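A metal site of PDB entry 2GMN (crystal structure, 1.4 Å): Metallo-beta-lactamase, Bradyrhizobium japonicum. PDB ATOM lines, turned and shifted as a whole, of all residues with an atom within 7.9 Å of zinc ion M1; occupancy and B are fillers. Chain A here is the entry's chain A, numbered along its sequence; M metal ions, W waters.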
ATOM      1  N   TRP A  14     -24.006  17.194  -7.324  1.00  0.00           N
ATOM      2  CA  TRP A  14     -22.797  16.393  -7.450  1.00  0.00           C
ATOM      3  C   TRP A  14     -22.725  15.210  -6.490  1.00  0.00           C
ATOM      4  O   TRP A  14     -22.007  14.242  -6.774  1.00  0.00           O
ATOM      5  CB  TRP A  14     -21.560  17.277  -7.281  1.00  0.00           C
ATOM      6  CG  TRP A  14     -21.270  18.146  -8.474  1.00  0.00           C
ATOM      7  CD1 TRP A  14     -22.087  18.372  -9.542  1.00  0.00           C
ATOM      8  CD2 TRP A  14     -20.086  18.918  -8.696  1.00  0.00           C
ATOM      9  NE1 TRP A  14     -21.472  19.233 -10.424  1.00  0.00           N
ATOM     10  CE2 TRP A  14     -20.256  19.586  -9.923  1.00  0.00           C
ATOM     11  CE3 TRP A  14     -18.903  19.113  -7.971  1.00  0.00           C
ATOM     12  CZ2 TRP A  14     -19.280  20.438 -10.458  1.00  0.00           C
ATOM     13  CZ3 TRP A  14     -17.932  19.974  -8.504  1.00  0.00           C
ATOM     14  CH2 TRP A  14     -18.125  20.607  -9.732  1.00  0.00           C
ATOM     15  N   GLY A  34     -24.719  14.274 -10.690  1.00  0.00           N
ATOM     16  CA  GLY A  34     -24.006  15.453 -11.190  1.00  0.00           C
ATOM     17  C   GLY A  34     -22.550  15.274 -11.600  1.00  0.00           C
ATOM     18  O   GLY A  34     -21.986  16.191 -12.179  1.00  0.00           O
ATOM     19  N   ILE A  35     -21.958  14.121 -11.283  1.00  0.00           N
ATOM     20  CA  ILE A  35     -20.585  13.784 -11.689  1.00  0.00           C
ATOM     21  C   ILE A  35     -20.622  12.413 -12.330  1.00  0.00           C
ATOM     22  O   ILE A  35     -21.128  11.454 -11.738  1.00  0.00           O
ATOM     23  CB  ILE A  35     -19.595  13.788 -10.490  1.00  0.00           C
ATOM     24  CG1 ILE A  35     -19.459  15.203  -9.923  1.00  0.00           C
ATOM     25  CG2 ILE A  35     -18.222  13.273 -10.915  1.00  0.00           C
ATOM     26  CD1 ILE A  35     -18.677  15.245  -8.603  1.00  0.00           C
ATOM     27  N   ALA A  36     -20.107  12.318 -13.554  1.00  0.00           N
ATOM     28  CA  ALA A  36     -20.108  11.064 -14.284  1.00  0.00           C
ATOM     29  C   ALA A  36     -18.848  10.250 -14.033  1.00  0.00           C
ATOM     30  O   ALA A  36     -17.715  10.763 -14.128  1.00  0.00           O
ATOM     31  CB  ALA A  36     -20.274  11.308 -15.749  1.00  0.00           C
ATOM     32  N   THR A  80      -9.846  11.909 -16.930  1.00  0.00           N
ATOM     33  CA  THR A  80     -10.102  12.932 -17.945  1.00  0.00           C
ATOM     34  C   THR A  80      -9.309  14.202 -17.595  1.00  0.00           C
ATOM     35  O   THR A  80      -8.523  14.696 -18.392  1.00  0.00           O
ATOM     36  CB  THR A  80     -11.602  13.293 -18.038  1.00  0.00           C
ATOM     37  OG1 THR A  80     -12.118  13.514 -16.719  1.00  0.00           O
ATOM     38  CG2 THR A  80     -12.384  12.198 -18.740  1.00  0.00           C
ATOM     39  N   HIS A  81      -9.509  14.735 -16.392  1.00  0.00           N
ATOM     40  CA  HIS A  81      -8.725  15.906 -15.977  1.00  0.00           C
ATOM     41  C   HIS A  81      -8.632  16.002 -14.463  1.00  0.00           C
ATOM     42  O   HIS A  81      -9.499  15.487 -13.753  1.00  0.00           O
ATOM     43  CB  HIS A  81      -9.264  17.199 -16.594  1.00  0.00           C
ATOM     44  CG  HIS A  81     -10.533  17.685 -15.962  1.00  0.00           C
ATOM     45  ND1 HIS A  81     -11.778  17.336 -16.442  1.00  0.00           N
ATOM     46  CD2 HIS A  81     -10.746  18.522 -14.921  1.00  0.00           C
ATOM     47  CE1 HIS A  81     -12.707  17.923 -15.699  1.00  0.00           C
ATOM     48  NE2 HIS A  81     -12.109  18.645 -14.769  1.00  0.00           N
ATOM     49  N   HIS A  83      -9.108  17.717 -11.609  1.00  0.00           N
ATOM     50  CA  HIS A  83      -9.797  18.537 -10.597  1.00  0.00           C
ATOM     51  C   HIS A  83     -10.462  17.640  -9.565  1.00  0.00           C
ATOM     52  O   HIS A  83     -10.825  16.500  -9.883  1.00  0.00           O
ATOM     53  CB  HIS A  83     -10.874  19.402 -11.224  1.00  0.00           C
ATOM     54  CG  HIS A  83     -10.348  20.509 -12.079  1.00  0.00           C
ATOM     55  ND1 HIS A  83     -11.107  21.092 -13.078  1.00  0.00           N
ATOM     56  CD2 HIS A  83      -9.148  21.141 -12.094  1.00  0.00           C
ATOM     57  CE1 HIS A  83     -10.389  22.051 -13.658  1.00  0.00           C
ATOM     58  NE2 HIS A  83      -9.194  22.083 -13.095  1.00  0.00           N
ATOM     59  N   LEU A  84     -10.659  18.157  -8.336  1.00  0.00           N
ATOM     60  CA  LEU A  84     -11.105  17.338  -7.209  1.00  0.00           C
ATOM     61  C   LEU A  84     -12.433  16.625  -7.426  1.00  0.00           C
ATOM     62  O   LEU A  84     -12.670  15.592  -6.816  1.00  0.00           O
ATOM     63  CB  LEU A  84     -11.159  18.152  -5.915  1.00  0.00           C
ATOM     64  CG  LEU A  84     -12.392  19.007  -5.625  1.00  0.00           C
ATOM     65  CD1 LEU A  84     -12.440  19.326  -4.142  1.00  0.00           C
ATOM     66  CD2 LEU A  84     -12.416  20.292  -6.472  1.00  0.00           C
ATOM     67  N   ASP A  85     -13.286  17.155  -8.301  1.00  0.00           N
ATOM     68  CA  ASP A  85     -14.589  16.519  -8.500  1.00  0.00           C
ATOM     69  C   ASP A  85     -14.477  15.260  -9.359  1.00  0.00           C
ATOM     70  O   ASP A  85     -15.456  14.524  -9.501  1.00  0.00           O
ATOM     71  CB  ASP A  85     -15.650  17.508  -9.032  1.00  0.00           C
ATOM     72  CG  ASP A  85     -15.219  18.246 -10.288  1.00  0.00           C
ATOM     73  OD1 ASP A  85     -14.045  18.687 -10.377  1.00  0.00           O
ATOM     74  OD2 ASP A  85     -16.082  18.424 -11.195  1.00  0.00           O
ATOM     75  N   HIS A  86     -13.290  15.019  -9.891  1.00  0.00           N
ATOM     76  CA  HIS A  86     -13.004  13.811 -10.691  1.00  0.00           C
ATOM     77  C   HIS A  86     -11.882  12.949 -10.127  1.00  0.00           C
ATOM     78  O   HIS A  86     -11.770  11.781 -10.471  1.00  0.00           O
ATOM     79  CB  HIS A  86     -12.705  14.182 -12.137  1.00  0.00           C
ATOM     80  CG  HIS A  86     -13.737  15.099 -12.693  1.00  0.00           C
ATOM     81  ND1 HIS A  86     -15.033  14.694 -12.939  1.00  0.00           N
ATOM     82  CD2 HIS A  86     -13.699  16.424 -12.963  1.00  0.00           C
ATOM     83  CE1 HIS A  86     -15.741  15.722 -13.360  1.00  0.00           C
ATOM     84  NE2 HIS A  86     -14.951  16.788 -13.384  1.00  0.00           N
ATOM     85  N   HIS A 157      -9.415  23.193 -20.147  1.00  0.00           N
ATOM     86  CA  HIS A 157     -10.073  23.117 -18.842  1.00  0.00           C
ATOM     87  C   HIS A 157      -9.041  22.734 -17.762  1.00  0.00           C
ATOM     88  O   HIS A 157      -9.124  23.166 -16.609  1.00  0.00           O
ATOM     89  CB  HIS A 157     -11.242  22.139 -18.893  1.00  0.00           C
ATOM     90  CG  HIS A 157     -11.991  22.044 -17.602  1.00  0.00           C
ATOM     91  ND1 HIS A 157     -13.004  22.919 -17.260  1.00  0.00           N
ATOM     92  CD2 HIS A 157     -11.861  21.182 -16.567  1.00  0.00           C
ATOM     93  CE1 HIS A 157     -13.462  22.602 -16.058  1.00  0.00           C
ATOM     94  NE2 HIS A 157     -12.780  21.556 -15.613  1.00  0.00           N
ATOM     95  N   CYS A 181     -13.057  15.318 -22.157  1.00  0.00           N
ATOM     96  CA  CYS A 181     -12.450  15.620 -20.861  1.00  0.00           C
ATOM     97  C   CYS A 181     -13.050  16.804 -20.102  1.00  0.00           C
ATOM     98  O   CYS A 181     -12.829  16.933 -18.905  1.00  0.00           O
ATOM     99  CB  CYS A 181     -10.938  15.801 -21.018  1.00  0.00           C
ATOM    100  SG  CYS A 181     -10.478  17.393 -21.688  1.00  0.00           S
ATOM    101  N   SER A 182     -13.767  17.653 -20.820  1.00  0.00           N
ATOM    102  CA  SER A 182     -14.382  18.919 -20.362  1.00  0.00           C
ATOM    103  C   SER A 182     -13.769  20.085 -21.129  1.00  0.00           C
ATOM    104  O   SER A 182     -12.548  20.137 -21.315  1.00  0.00           O
ATOM    105  CB  SER A 182     -14.260  19.207 -18.868  1.00  0.00           C
ATOM    106  OG  SER A 182     -14.818  20.481 -18.625  1.00  0.00           O
ATOM    107  N   THR A 184     -15.341  23.426 -20.409  1.00  0.00           N
ATOM    108  CA  THR A 184     -15.952  24.584 -19.766  1.00  0.00           C
ATOM    109  C   THR A 184     -14.887  25.522 -19.211  1.00  0.00           C
ATOM    110  O   THR A 184     -13.757  25.105 -18.929  1.00  0.00           O
ATOM    111  CB  THR A 184     -16.839  24.150 -18.601  1.00  0.00           C
ATOM    112  OG1 THR A 184     -16.046  23.426 -17.657  1.00  0.00           O
ATOM    113  CG2 THR A 184     -17.981  23.240 -19.101  1.00  0.00           C
ATOM    114  N   ALA A 186     -15.523  27.406 -16.350  1.00  0.00           N
ATOM    115  CA  ALA A 186     -15.704  27.122 -14.924  1.00  0.00           C
ATOM    116  C   ALA A 186     -14.885  28.096 -14.061  1.00  0.00           C
ATOM    117  O   ALA A 186     -15.079  29.313 -14.165  1.00  0.00           O
ATOM    118  CB  ALA A 186     -15.361  25.655 -14.636  1.00  0.00           C
ATOM    119  N   PRO A 221     -17.306  14.096 -18.206  1.00  0.00           N
ATOM    120  CA  PRO A 221     -17.153  13.917 -16.755  1.00  0.00           C
ATOM    121  C   PRO A 221     -18.292  14.463 -15.889  1.00  0.00           C
ATOM    122  O   PRO A 221     -18.300  14.254 -14.667  1.00  0.00           O
ATOM    123  CB  PRO A 221     -15.825  14.624 -16.459  1.00  0.00           C
ATOM    124  CG  PRO A 221     -15.594  15.565 -17.592  1.00  0.00           C
ATOM    125  CD  PRO A 221     -16.509  15.219 -18.725  1.00  0.00           C
ATOM    126  N   HIS A 222     -19.260  15.132 -16.516  1.00  0.00           N
ATOM    127  CA  HIS A 222     -20.512  15.499 -15.876  1.00  0.00           C
ATOM    128  C   HIS A 222     -21.638  15.095 -16.816  1.00  0.00           C
ATOM    129  O   HIS A 222     -21.495  15.233 -18.030  1.00  0.00           O
ATOM    130  CB  HIS A 222     -20.541  17.015 -15.623  1.00  0.00           C
ATOM    131  CG  HIS A 222     -19.516  17.472 -14.637  1.00  0.00           C
ATOM    132  ND1 HIS A 222     -19.719  17.383 -13.268  1.00  0.00           N
ATOM    133  CD2 HIS A 222     -18.291  18.024 -14.801  1.00  0.00           C
ATOM    134  CE1 HIS A 222     -18.652  17.850 -12.641  1.00  0.00           C
ATOM    135  NE2 HIS A 222     -17.773  18.245 -13.547  1.00  0.00           N
HETATM  136 ZN    ZN M   1     -15.789  18.700 -13.201  1.00  0.00          ZN
HETATM  137 ZN    ZN M   2     -12.880  20.401 -13.939  1.00  0.00          ZN
HETATM  138  O   HOH W   1     -14.328  20.069 -12.653  1.00  0.00           O
HETATM  139  O   HOH W   2     -15.583  19.564 -15.581  1.00  0.00           O
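O of Gly 34 lies within hydrogen-bond range of ND1 of His 222, at 2.8 Å.
Within 4 Å of zinc ion M1: Asp 85, His 86 and His 222.
Zinc ion M1 is bound by the side-chain carboxylate (OD2) of Asp 85 (2.0 Å), a ring nitrogen (NE2) of His 222 (2.1 Å), water W1 (2.1 Å), a ring nitrogen (NE2) of His 86 (2.1 Å) and water W2 (2.5 Å).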
